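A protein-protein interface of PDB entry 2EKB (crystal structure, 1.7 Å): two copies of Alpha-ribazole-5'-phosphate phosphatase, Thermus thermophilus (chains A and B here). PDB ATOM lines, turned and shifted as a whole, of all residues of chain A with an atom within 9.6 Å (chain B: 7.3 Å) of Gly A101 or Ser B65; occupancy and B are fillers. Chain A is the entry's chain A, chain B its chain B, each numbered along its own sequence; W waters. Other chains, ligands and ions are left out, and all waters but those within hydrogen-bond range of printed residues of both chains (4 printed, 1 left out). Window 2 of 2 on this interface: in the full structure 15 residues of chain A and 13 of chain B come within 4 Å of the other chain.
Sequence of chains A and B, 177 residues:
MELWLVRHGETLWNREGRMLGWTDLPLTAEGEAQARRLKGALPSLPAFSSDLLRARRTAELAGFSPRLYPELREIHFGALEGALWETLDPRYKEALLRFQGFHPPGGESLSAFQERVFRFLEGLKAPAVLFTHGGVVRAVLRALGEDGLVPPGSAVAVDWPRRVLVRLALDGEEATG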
ATOM      1  N   ILE A  75      27.260  29.737  12.880  1.00  0.00           N
ATOM      2  CA  ILE A  75      26.116  30.637  12.826  1.00  0.00           C
ATOM      3  C   ILE A  75      26.463  31.927  13.578  1.00  0.00           C
ATOM      4  O   ILE A  75      27.249  31.910  14.528  1.00  0.00           O
ATOM      5  CB  ILE A  75      24.872  29.985  13.474  1.00  0.00           C
ATOM      6  CG1 ILE A  75      23.647  30.879  13.282  1.00  0.00           C
ATOM      7  CG2 ILE A  75      25.128  29.739  14.959  1.00  0.00           C
ATOM      8  CD1 ILE A  75      22.332  30.196  13.645  1.00  0.00           C
ATOM      9  N   LEU A  80      23.760  37.208  21.274  1.00  0.00           N
ATOM     10  CA  LEU A  80      24.069  36.054  22.108  1.00  0.00           C
ATOM     11  C   LEU A  80      25.542  35.656  22.037  1.00  0.00           C
ATOM     12  O   LEU A  80      25.985  34.785  22.779  1.00  0.00           O
ATOM     13  CB  LEU A  80      23.183  34.858  21.732  1.00  0.00           C
ATOM     14  CG  LEU A  80      21.684  35.045  21.996  1.00  0.00           C
ATOM     15  CD1 LEU A  80      20.937  33.762  21.640  1.00  0.00           C
ATOM     16  CD2 LEU A  80      21.461  35.406  23.461  1.00  0.00           C
ATOM     17  N   PRO A  90      15.385  30.157  28.212  1.00  0.00           N
ATOM     18  CA  PRO A  90      14.854  28.865  27.767  1.00  0.00           C
ATOM     19  C   PRO A  90      14.397  28.836  26.307  1.00  0.00           C
ATOM     20  O   PRO A  90      14.565  27.823  25.628  1.00  0.00           O
ATOM     21  CB  PRO A  90      13.711  28.617  28.744  1.00  0.00           C
ATOM     22  CG  PRO A  90      14.259  29.183  30.011  1.00  0.00           C
ATOM     23  CD  PRO A  90      14.869  30.498  29.550  1.00  0.00           C
ATOM     24  N   ARG A  91      13.827  29.937  25.823  1.00  0.00           N
ATOM     25  CA  ARG A  91      13.364  29.987  24.438  1.00  0.00           C
ATOM     26  C   ARG A  91      14.523  29.740  23.476  1.00  0.00           C
ATOM     27  O   ARG A  91      14.368  29.037  22.475  1.00  0.00           O
ATOM     28  CB  ARG A  91      12.713  31.337  24.123  1.00  0.00           C
ATOM     29  CG  ARG A  91      13.594  32.537  24.399  1.00  0.00           C
ATOM     30  CD  ARG A  91      12.953  33.818  23.900  1.00  0.00           C
ATOM     31  NE  ARG A  91      13.700  34.995  24.331  1.00  0.00           N
ATOM     32  CZ  ARG A  91      13.541  36.211  23.819  1.00  0.00           C
ATOM     33  NH1 ARG A  91      12.660  36.414  22.849  1.00  0.00           N
ATOM     34  NH2 ARG A  91      14.264  37.223  24.279  1.00  0.00           N
ATOM     35  N   TYR A  92      15.680  30.325  23.777  1.00  0.00           N
ATOM     36  CA  TYR A  92      16.852  30.138  22.933  1.00  0.00           C
ATOM     37  C   TYR A  92      17.422  28.743  23.130  1.00  0.00           C
ATOM     38  O   TYR A  92      17.785  28.077  22.165  1.00  0.00           O
ATOM     39  CB  TYR A  92      17.929  31.178  23.253  1.00  0.00           C
ATOM     40  CG  TYR A  92      17.559  32.582  22.851  1.00  0.00           C
ATOM     41  CD1 TYR A  92      17.109  32.861  21.561  1.00  0.00           C
ATOM     42  CD2 TYR A  92      17.675  33.640  23.752  1.00  0.00           C
ATOM     43  CE1 TYR A  92      16.783  34.157  21.177  1.00  0.00           C
ATOM     44  CE2 TYR A  92      17.354  34.940  23.379  1.00  0.00           C
ATOM     45  CZ  TYR A  92      16.908  35.191  22.091  1.00  0.00           C
ATOM     46  OH  TYR A  92      16.584  36.474  21.720  1.00  0.00           O
ATOM     47  N   LYS A  93      17.503  28.302  24.383  1.00  0.00           N
ATOM     48  CA  LYS A  93      18.024  26.974  24.682  1.00  0.00           C
ATOM     49  C   LYS A  93      17.235  25.915  23.929  1.00  0.00           C
ATOM     50  O   LYS A  93      17.812  25.063  23.251  1.00  0.00           O
ATOM     51  CB  LYS A  93      17.943  26.674  26.182  1.00  0.00           C
ATOM     52  CG  LYS A  93      19.104  27.185  27.015  1.00  0.00           C
ATOM     53  CD  LYS A  93      19.192  26.376  28.307  1.00  0.00           C
ATOM     54  CE  LYS A  93      20.297  26.870  29.229  1.00  0.00           C
ATOM     55  NZ  LYS A  93      19.944  28.170  29.856  1.00  0.00           N
ATOM     56  N   GLU A  94      15.911  25.975  24.048  1.00  0.00           N
ATOM     57  CA  GLU A  94      15.053  25.004  23.383  1.00  0.00           C
ATOM     58  C   GLU A  94      15.212  25.090  21.872  1.00  0.00           C
ATOM     59  O   GLU A  94      15.260  24.064  21.188  1.00  0.00           O
ATOM     60  CB  GLU A  94      13.586  25.233  23.760  1.00  0.00           C
ATOM     61  CG  GLU A  94      12.667  24.104  23.315  1.00  0.00           C
ATOM     62  CD  GLU A  94      11.220  24.331  23.711  1.00  0.00           C
ATOM     63  OE1 GLU A  94      10.579  25.242  23.143  1.00  0.00           O
ATOM     64  OE2 GLU A  94      10.728  23.599  24.598  1.00  0.00           O
ATOM     65  N   ALA A  95      15.290  26.313  21.355  1.00  0.00           N
ATOM     66  CA  ALA A  95      15.445  26.518  19.919  1.00  0.00           C
ATOM     67  C   ALA A  95      16.720  25.842  19.424  1.00  0.00           C
ATOM     68  O   ALA A  95      16.715  25.173  18.392  1.00  0.00           O
ATOM     69  CB  ALA A  95      15.482  28.014  19.596  1.00  0.00           C
ATOM     70  N   LEU A  96      17.811  26.020  20.164  1.00  0.00           N
ATOM     71  CA  LEU A  96      19.084  25.425  19.788  1.00  0.00           C
ATOM     72  C   LEU A  96      19.093  23.911  20.002  1.00  0.00           C
ATOM     73  O   LEU A  96      19.640  23.167  19.188  1.00  0.00           O
ATOM     74  CB  LEU A  96      20.223  26.087  20.573  1.00  0.00           C
ATOM     75  CG  LEU A  96      20.491  27.544  20.181  1.00  0.00           C
ATOM     76  CD1 LEU A  96      21.540  28.156  21.099  1.00  0.00           C
ATOM     77  CD2 LEU A  96      20.941  27.604  18.727  1.00  0.00           C
ATOM     78  N   LEU A  97      18.489  23.450  21.092  1.00  0.00           N
ATOM     79  CA  LEU A  97      18.444  22.014  21.354  1.00  0.00           C
ATOM     80  C   LEU A  97      17.620  21.299  20.286  1.00  0.00           C
ATOM     81  O   LEU A  97      17.991  20.224  19.818  1.00  0.00           O
ATOM     82  CB  LEU A  97      17.851  21.742  22.740  1.00  0.00           C
ATOM     83  CG  LEU A  97      18.705  22.201  23.923  1.00  0.00           C
ATOM     84  CD1 LEU A  97      17.958  21.936  25.219  1.00  0.00           C
ATOM     85  CD2 LEU A  97      20.045  21.468  23.915  1.00  0.00           C
ATOM     86  N   ARG A  98      16.503  21.902  19.897  1.00  0.00           N
ATOM     87  CA  ARG A  98      15.637  21.314  18.882  1.00  0.00           C
ATOM     88  C   ARG A  98      16.037  21.764  17.476  1.00  0.00           C
ATOM     89  O   ARG A  98      15.418  21.355  16.491  1.00  0.00           O
ATOM     90  CB  ARG A  98      14.178  21.692  19.153  1.00  0.00           C
ATOM     91  CG  ARG A  98      13.637  21.168  20.474  1.00  0.00           C
ATOM     92  CD  ARG A  98      12.185  21.575  20.670  1.00  0.00           C
ATOM     93  NE  ARG A  98      11.312  21.009  19.645  1.00  0.00           N
ATOM     94  CZ  ARG A  98      11.043  19.713  19.523  1.00  0.00           C
ATOM     95  NH1 ARG A  98      11.576  18.840  20.368  1.00  0.00           N
ATOM     96  NH2 ARG A  98      10.245  19.286  18.552  1.00  0.00           N
ATOM     97  N   PHE A  99      17.065  22.608  17.399  1.00  0.00           N
ATOM     98  CA  PHE A  99      17.582  23.125  16.130  1.00  0.00           C
ATOM     99  C   PHE A  99      16.449  23.639  15.240  1.00  0.00           C
ATOM    100  O   PHE A  99      16.282  23.188  14.105  1.00  0.00           O
ATOM    101  CB  PHE A  99      18.361  22.025  15.394  1.00  0.00           C
ATOM    102  CG  PHE A  99      19.592  22.520  14.674  1.00  0.00           C
ATOM    103  CD1 PHE A  99      20.654  23.068  15.385  1.00  0.00           C
ATOM    104  CD2 PHE A  99      19.696  22.421  13.287  1.00  0.00           C
ATOM    105  CE1 PHE A  99      21.810  23.511  14.728  1.00  0.00           C
ATOM    106  CE2 PHE A  99      20.844  22.861  12.618  1.00  0.00           C
ATOM    107  CZ  PHE A  99      21.902  23.406  13.338  1.00  0.00           C
ATOM    108  N   GLN A 100      15.684  24.602  15.747  1.00  0.00           N
ATOM    109  CA  GLN A 100      14.564  25.153  14.990  1.00  0.00           C
ATOM    110  C   GLN A 100      14.097  26.483  15.578  1.00  0.00           C
ATOM    111  O   GLN A 100      14.227  26.720  16.779  1.00  0.00           O
ATOM    112  CB  GLN A 100      13.396  24.167  15.018  1.00  0.00           C
ATOM    113  CG  GLN A 100      12.841  23.970  16.416  1.00  0.00           C
ATOM    114  CD  GLN A 100      11.698  22.980  16.481  1.00  0.00           C
ATOM    115  OE1 GLN A 100      11.128  22.751  17.548  1.00  0.00           O
ATOM    116  NE2 GLN A 100      11.363  22.382  15.346  1.00  0.00           N
ATOM    117  N   GLY A 101      13.547  27.338  14.721  1.00  0.00           N
ATOM    118  CA  GLY A 101      13.034  28.624  15.165  1.00  0.00           C
ATOM    119  C   GLY A 101      13.961  29.397  16.079  1.00  0.00           C
ATOM    120  O   GLY A 101      13.591  29.768  17.195  1.00  0.00           O
ATOM    121  N   PHE A 102      15.172  29.645  15.598  1.00  0.00           N
ATOM    122  CA  PHE A 102      16.172  30.382  16.356  1.00  0.00           C
ATOM    123  C   PHE A 102      16.507  31.668  15.613  1.00  0.00           C
ATOM    124  O   PHE A 102      17.027  31.628  14.497  1.00  0.00           O
ATOM    125  CB  PHE A 102      17.437  29.535  16.508  1.00  0.00           C
ATOM    126  CG  PHE A 102      18.572  30.243  17.199  1.00  0.00           C
ATOM    127  CD1 PHE A 102      18.464  30.634  18.526  1.00  0.00           C
ATOM    128  CD2 PHE A 102      19.765  30.491  16.522  1.00  0.00           C
ATOM    129  CE1 PHE A 102      19.530  31.257  19.174  1.00  0.00           C
ATOM    130  CE2 PHE A 102      20.834  31.113  17.158  1.00  0.00           C
ATOM    131  CZ  PHE A 102      20.717  31.496  18.487  1.00  0.00           C
ATOM    132  N   HIS A 103      16.190  32.809  16.215  1.00  0.00           N
ATOM    133  CA  HIS A 103      16.494  34.080  15.578  1.00  0.00           C
ATOM    134  C   HIS A 103      17.008  35.075  16.602  1.00  0.00           C
ATOM    135  O   HIS A 103      16.246  35.864  17.169  1.00  0.00           O
ATOM    136  CB  HIS A 103      15.270  34.664  14.870  1.00  0.00           C
ATOM    137  CG  HIS A 103      15.622  35.549  13.713  1.00  0.00           C
ATOM    138  ND1 HIS A 103      16.724  36.380  13.725  1.00  0.00           N
ATOM    139  CD2 HIS A 103      15.030  35.727  12.510  1.00  0.00           C
ATOM    140  CE1 HIS A 103      16.794  37.029  12.576  1.00  0.00           C
ATOM    141  NE2 HIS A 103      15.778  36.651  11.821  1.00  0.00           N
ATOM    142  N   PRO A 104      18.317  35.042  16.858  1.00  0.00           N
ATOM    143  CA  PRO A 104      18.944  35.946  17.822  1.00  0.00           C
ATOM    144  C   PRO A 104      18.992  37.378  17.302  1.00  0.00           C
ATOM    145  O   PRO A 104      19.310  37.617  16.133  1.00  0.00           O
ATOM    146  CB  PRO A 104      20.334  35.341  17.994  1.00  0.00           C
ATOM    147  CG  PRO A 104      20.619  34.797  16.638  1.00  0.00           C
ATOM    148  CD  PRO A 104      19.313  34.129  16.270  1.00  0.00           C
ATOM    149  N   GLU A 108      21.991  35.859  12.976  1.00  0.00           N
ATOM    150  CA  GLU A 108      21.530  35.096  11.826  1.00  0.00           C
ATOM    151  C   GLU A 108      20.553  34.014  12.292  1.00  0.00           C
ATOM    152  O   GLU A 108      20.804  33.335  13.287  1.00  0.00           O
ATOM    153  CB  GLU A 108      22.769  34.485  11.172  1.00  0.00           C
ATOM    154  CG  GLU A 108      22.579  33.639   9.949  1.00  0.00           C
ATOM    155  CD  GLU A 108      23.927  33.234   9.375  1.00  0.00           C
ATOM    156  OE1 GLU A 108      24.835  32.923  10.177  1.00  0.00           O
ATOM    157  OE2 GLU A 108      24.079  33.232   8.136  1.00  0.00           O
ATOM    158  N   SER A 109      19.436  33.865  11.588  1.00  0.00           N
ATOM    159  CA  SER A 109      18.449  32.855  11.958  1.00  0.00           C
ATOM    160  C   SER A 109      18.973  31.482  11.555  1.00  0.00           C
ATOM    161  O   SER A 109      19.810  31.365  10.656  1.00  0.00           O
ATOM    162  CB  SER A 109      17.115  33.108  11.252  1.00  0.00           C
ATOM    163  OG  SER A 109      17.198  32.798   9.871  1.00  0.00           O
ATOM    164  N   LEU A 110      18.476  30.444  12.218  1.00  0.00           N
ATOM    165  CA  LEU A 110      18.912  29.090  11.910  1.00  0.00           C
ATOM    166  C   LEU A 110      18.566  28.768  10.463  1.00  0.00           C
ATOM    167  O   LEU A 110      19.338  28.104   9.771  1.00  0.00           O
ATOM    168  CB  LEU A 110      18.235  28.086  12.839  1.00  0.00           C
ATOM    169  CG  LEU A 110      18.731  26.648  12.702  1.00  0.00           C
ATOM    170  CD1 LEU A 110      20.197  26.577  13.097  1.00  0.00           C
ATOM    171  CD2 LEU A 110      17.906  25.740  13.596  1.00  0.00           C
ATOM    172  N   SER A 111      17.408  29.245  10.011  1.00  0.00           N
ATOM    173  CA  SER A 111      16.972  29.011   8.635  1.00  0.00           C
ATOM    174  C   SER A 111      17.943  29.626   7.631  1.00  0.00           C
ATOM    175  O   SER A 111      18.279  29.005   6.622  1.00  0.00           O
ATOM    176  CB  SER A 111      15.564  29.585   8.415  1.00  0.00           C
ATOM    177  OG  SER A 111      14.595  28.820   9.109  1.00  0.00           O
ATOM    178  N   ALA A 112      18.392  30.849   7.909  1.00  0.00           N
ATOM    179  CA  ALA A 112      19.331  31.527   7.021  1.00  0.00           C
ATOM    180  C   ALA A 112      20.681  30.825   7.069  1.00  0.00           C
ATOM    181  O   ALA A 112      21.381  30.737   6.066  1.00  0.00           O
ATOM    182  CB  ALA A 112      19.486  32.988   7.429  1.00  0.00           C
ATOM    183  N   GLN A 114      21.217  27.566   7.719  1.00  0.00           N
ATOM    184  CA  GLN A 114      21.108  26.335   6.944  1.00  0.00           C
ATOM    185  C   GLN A 114      21.155  26.626   5.447  1.00  0.00           C
ATOM    186  O   GLN A 114      21.882  25.963   4.709  1.00  0.00           O
ATOM    187  CB  GLN A 114      19.811  25.593   7.296  1.00  0.00           C
ATOM    188  CG  GLN A 114      19.819  24.980   8.689  1.00  0.00           C
ATOM    189  CD  GLN A 114      18.445  24.507   9.116  1.00  0.00           C
ATOM    190  OE1 GLN A 114      17.445  25.183   8.870  1.00  0.00           O
ATOM    191  NE2 GLN A 114      18.385  23.348   9.769  1.00  0.00           N
ATOM    192  N   PRO B  46      15.322  19.788   8.327  1.00  0.00           N
ATOM    193  CA  PRO B  46      14.893  21.166   8.065  1.00  0.00           C
ATOM    194  C   PRO B  46      13.433  21.087   7.618  1.00  0.00           C
ATOM    195  O   PRO B  46      13.071  20.202   6.833  1.00  0.00           O
ATOM    196  CB  PRO B  46      15.816  21.603   6.930  1.00  0.00           C
ATOM    197  CG  PRO B  46      17.090  20.876   7.247  1.00  0.00           C
ATOM    198  CD  PRO B  46      16.597  19.491   7.642  1.00  0.00           C
ATOM    199  N   ALA B  47      12.598  21.999   8.108  1.00  0.00           N
ATOM    200  CA  ALA B  47      11.186  21.966   7.760  1.00  0.00           C
ATOM    201  C   ALA B  47      10.717  23.123   6.889  1.00  0.00           C
ATOM    202  O   ALA B  47      11.212  24.247   6.994  1.00  0.00           O
ATOM    203  CB  ALA B  47      10.356  21.906   9.034  1.00  0.00           C
ATOM    204  N   PHE B  48       9.750  22.822   6.029  1.00  0.00           N
ATOM    205  CA  PHE B  48       9.151  23.796   5.126  1.00  0.00           C
ATOM    206  C   PHE B  48       7.661  23.526   5.176  1.00  0.00           C
ATOM    207  O   PHE B  48       7.233  22.407   5.478  1.00  0.00           O
ATOM    208  CB  PHE B  48       9.650  23.599   3.691  1.00  0.00           C
ATOM    209  CG  PHE B  48      11.119  23.838   3.520  1.00  0.00           C
ATOM    210  CD1 PHE B  48      12.034  22.826   3.790  1.00  0.00           C
ATOM    211  CD2 PHE B  48      11.595  25.081   3.111  1.00  0.00           C
ATOM    212  CE1 PHE B  48      13.405  23.045   3.658  1.00  0.00           C
ATOM    213  CE2 PHE B  48      12.963  25.313   2.973  1.00  0.00           C
ATOM    214  CZ  PHE B  48      13.872  24.291   3.249  1.00  0.00           C
ATOM    215  N   SER B  49       6.861  24.539   4.882  1.00  0.00           N
ATOM    216  CA  SER B  49       5.426  24.343   4.922  1.00  0.00           C
ATOM    217  C   SER B  49       4.677  25.289   4.014  1.00  0.00           C
ATOM    218  O   SER B  49       5.130  26.400   3.728  1.00  0.00           O
ATOM    219  CB  SER B  49       4.909  24.535   6.355  1.00  0.00           C
ATOM    220  OG  SER B  49       3.487  24.459   6.414  1.00  0.00           O
ATOM    221  N   ALA B  59       2.377  21.643  11.184  1.00  0.00           N
ATOM    222  CA  ALA B  59       3.815  21.677  11.436  1.00  0.00           C
ATOM    223  C   ALA B  59       4.079  22.047  12.893  1.00  0.00           C
ATOM    224  O   ALA B  59       4.876  21.399  13.578  1.00  0.00           O
ATOM    225  CB  ALA B  59       4.491  22.685  10.509  1.00  0.00           C
ATOM    226  N   GLU B  60       3.401  23.085  13.368  1.00  0.00           N
ATOM    227  CA  GLU B  60       3.574  23.538  14.749  1.00  0.00           C
ATOM    228  C   GLU B  60       3.250  22.460  15.780  1.00  0.00           C
ATOM    229  O   GLU B  60       4.029  22.214  16.705  1.00  0.00           O
ATOM    230  CB  GLU B  60       2.708  24.773  15.013  1.00  0.00           C
ATOM    231  CG  GLU B  60       2.757  25.266  16.450  1.00  0.00           C
ATOM    232  CD  GLU B  60       1.969  26.545  16.652  1.00  0.00           C
ATOM    233  OE1 GLU B  60       0.807  26.604  16.202  1.00  0.00           O
ATOM    234  OE2 GLU B  60       2.513  27.488  17.267  1.00  0.00           O
ATOM    235  N   ALA B  62       3.248  19.380  15.306  1.00  0.00           N
ATOM    236  CA  ALA B  62       4.144  18.239  15.127  1.00  0.00           C
ATOM    237  C   ALA B  62       5.551  18.521  15.672  1.00  0.00           C
ATOM    238  O   ALA B  62       6.447  17.691  15.621  1.00  0.00           O
ATOM    239  CB  ALA B  62       4.219  17.899  13.638  1.00  0.00           C
ATOM    240  N   GLY B  63       5.736  19.768  16.154  1.00  0.00           N
ATOM    241  CA  GLY B  63       7.000  20.121  16.811  1.00  0.00           C
ATOM    242  C   GLY B  63       8.013  20.790  15.872  1.00  0.00           C
ATOM    243  O   GLY B  63       9.214  20.769  16.108  1.00  0.00           O
ATOM    244  N   PHE B  64       7.548  21.411  14.792  1.00  0.00           N
ATOM    245  CA  PHE B  64       8.432  22.072  13.833  1.00  0.00           C
ATOM    246  C   PHE B  64       8.173  23.574  13.719  1.00  0.00           C
ATOM    247  O   PHE B  64       7.100  24.059  14.080  1.00  0.00           O
ATOM    248  CB  PHE B  64       8.256  21.447  12.443  1.00  0.00           C
ATOM    249  CG  PHE B  64       8.720  20.020  12.350  1.00  0.00           C
ATOM    250  CD1 PHE B  64       7.892  18.980  12.760  1.00  0.00           C
ATOM    251  CD2 PHE B  64       9.987  19.718  11.861  1.00  0.00           C
ATOM    252  CE1 PHE B  64       8.320  17.653  12.686  1.00  0.00           C
ATOM    253  CE2 PHE B  64      10.426  18.393  11.780  1.00  0.00           C
ATOM    254  CZ  PHE B  64       9.592  17.362  12.193  1.00  0.00           C
ATOM    255  N   SER B  65       9.173  24.291  13.210  1.00  0.00           N
ATOM    256  CA  SER B  65       9.109  25.739  12.980  1.00  0.00           C
ATOM    257  C   SER B  65       9.563  25.848  11.528  1.00  0.00           C
ATOM    258  O   SER B  65      10.719  26.145  11.235  1.00  0.00           O
ATOM    259  CB  SER B  65      10.085  26.479  13.900  1.00  0.00           C
ATOM    260  OG  SER B  65       9.757  26.259  15.259  1.00  0.00           O
ATOM    261  N   PRO B  66       8.638  25.617  10.592  1.00  0.00           N
ATOM    262  CA  PRO B  66       8.913  25.656   9.154  1.00  0.00           C
ATOM    263  C   PRO B  66       9.109  26.985   8.442  1.00  0.00           C
ATOM    264  O   PRO B  66       8.579  28.018   8.849  1.00  0.00           O
ATOM    265  CB  PRO B  66       7.720  24.905   8.576  1.00  0.00           C
ATOM    266  CG  PRO B  66       6.608  25.416   9.439  1.00  0.00           C
ATOM    267  CD  PRO B  66       7.211  25.343  10.843  1.00  0.00           C
ATOM    268  N   ARG B  67       9.888  26.927   7.366  1.00  0.00           N
ATOM    269  CA  ARG B  67      10.102  28.075   6.497  1.00  0.00           C
ATOM    270  C   ARG B  67       8.857  27.992   5.618  1.00  0.00           C
ATOM    271  O   ARG B  67       8.508  26.908   5.138  1.00  0.00           O
ATOM    272  CB  ARG B  67      11.370  27.887   5.658  1.00  0.00           C
ATOM    273  CG  ARG B  67      12.658  28.073   6.455  1.00  0.00           C
ATOM    274  CD  ARG B  67      13.887  27.575   5.703  1.00  0.00           C
ATOM    275  NE  ARG B  67      14.107  28.271   4.439  1.00  0.00           N
ATOM    276  CZ  ARG B  67      15.154  28.060   3.645  1.00  0.00           C
ATOM    277  NH1 ARG B  67      16.080  27.169   3.984  1.00  0.00           N
ATOM    278  NH2 ARG B  67      15.275  28.734   2.511  1.00  0.00           N
ATOM    279  N   LEU B  68       8.174  29.118   5.420  1.00  0.00           N
ATOM    280  CA  LEU B  68       6.949  29.128   4.631  1.00  0.00           C
ATOM    281  C   LEU B  68       7.143  29.414   3.146  1.00  0.00           C
ATOM    282  O   LEU B  68       7.834  30.358   2.757  1.00  0.00           O
ATOM    283  CB  LEU B  68       5.956  30.134   5.237  1.00  0.00           C
ATOM    284  CG  LEU B  68       5.646  29.965   6.730  1.00  0.00           C
ATOM    285  CD1 LEU B  68       4.560  30.962   7.150  1.00  0.00           C
ATOM    286  CD2 LEU B  68       5.183  28.544   7.005  1.00  0.00           C
ATOM    287  N   PHE B 131       5.489  20.137   5.064  1.00  0.00           N
ATOM    288  CA  PHE B 131       4.089  20.131   5.494  1.00  0.00           C
ATOM    289  C   PHE B 131       3.295  20.719   4.346  1.00  0.00           C
ATOM    290  O   PHE B 131       3.421  21.901   4.025  1.00  0.00           O
ATOM    291  CB  PHE B 131       3.953  20.952   6.772  1.00  0.00           C
ATOM    292  CG  PHE B 131       4.569  20.281   7.948  1.00  0.00           C
ATOM    293  CD1 PHE B 131       3.861  19.319   8.656  1.00  0.00           C
ATOM    294  CD2 PHE B 131       5.898  20.523   8.285  1.00  0.00           C
ATOM    295  CE1 PHE B 131       4.462  18.597   9.676  1.00  0.00           C
ATOM    296  CE2 PHE B 131       6.511  19.805   9.309  1.00  0.00           C
ATOM    297  CZ  PHE B 131       5.789  18.837  10.004  1.00  0.00           C
HETATM  298  O   HOH W   1      11.791  22.735  12.443  1.00  0.00           O
HETATM  299  O   HOH W   2      13.453  26.035  11.977  1.00  0.00           O
HETATM  300  O   HOH W   3       9.208  17.341  16.025  1.00  0.00           O
HETATM  301  O   HOH W   4      16.156  25.437   6.368  1.00  0.00           O
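The guanidinium group of Arg A98 sits at hydrogen-bond distance from the backbone carbonyl oxygen of Gly B63 (3.0 Å).
NE2 of Gln A100 lies within hydrogen-bond range of O of Gly B63, 2.8 Å away.
The backbone carbonyl oxygen (O) of Ala A95 sits at hydrogen-bond distance from the backbone NH (N) of Gln A100, 2.9 Å away.
NE of Arg A98 is in hydrogen-bond range of OE1 of Gln A100, at 2.7 Å.
The backbone carbonyl oxygen of Ala B47 lies within hydrogen-bond range of the backbone NH of Arg B67 (3.0 Å).
The backbone carbonyl oxygen (O) of Arg B67 lies within hydrogen-bond range of the backbone NH (N) of Ser B49.
The backbone carbonyl oxygen (O) of Ala B59 lies within hydrogen-bond range of the backbone NH (N) of Phe B64, at 2.9 Å.
Among the printed residues, merely in contact across the chains: Gln A100 with Phe B64 (3.3 Å), Ser A111 with Arg B67 (3.4 Å), Gln A100 with Ser B65 (3.6 Å), Gly A101 with Ser B65 (3.7 Å) and Gln A114 with Pro B46 (3.8 Å).
Ser B65 touches two residues of chain A.
No residue of chain A comes within 4 Å of Pro B66.
Printed residues of chain A within 4 Å of Pro B46: Gln A114.
Of the printed residues of chain A, Phe B64 touches Gln A100 (3.3 Å).
Printed residues of chain A within 4 Å of Gly B63: Arg A98 (3.0 Å) and Gln A100 (2.8 Å).
Printed residues of chain B within 4 Å of Gln A114: Pro B46 (3.8 Å).
Of the printed residues of chain B, Arg A98 touches Gly B63.
The nearest printed residue of chain B that does not touch Gly A101 is Phe B64 (6.6 Å).
The nearest residue of chain A that does not touch Ser B65 is Ser A111 (5.2 Å).
Of the 23 printed residues of chain A, 5 touch a printed residue of chain B.
Printed residues of chain A that touch a printed residue of chain B: Arg A98, Gln A100, Gly A101, Ser A111 and Gln A114.
Among the printed residues, 7 pairs touch across the chains.
Among the printed residues, no Asp or Glu carboxylate lies within 4 Å of a Lys or Arg side-chain nitrogen of the other chain.
No position is printed for both chains.
Of the 7 pairs that touch across the chains among the printed residues, none has its exchanged pair printed and touching as well.
Water W3 lies within hydrogen-bond range of O of Ala B62, NH2 of Arg A98 and O of Gly B63.
Water W4 lies within hydrogen-bond range of OE1 of Gln A114 (2.8 Å) and NH1 of Arg B67 (2.9 Å).
Water W2 bridges O of Ser B65 and N of Gly A101.
Water W1 bridges NE2 of Gln A100 and N of Ser B65.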
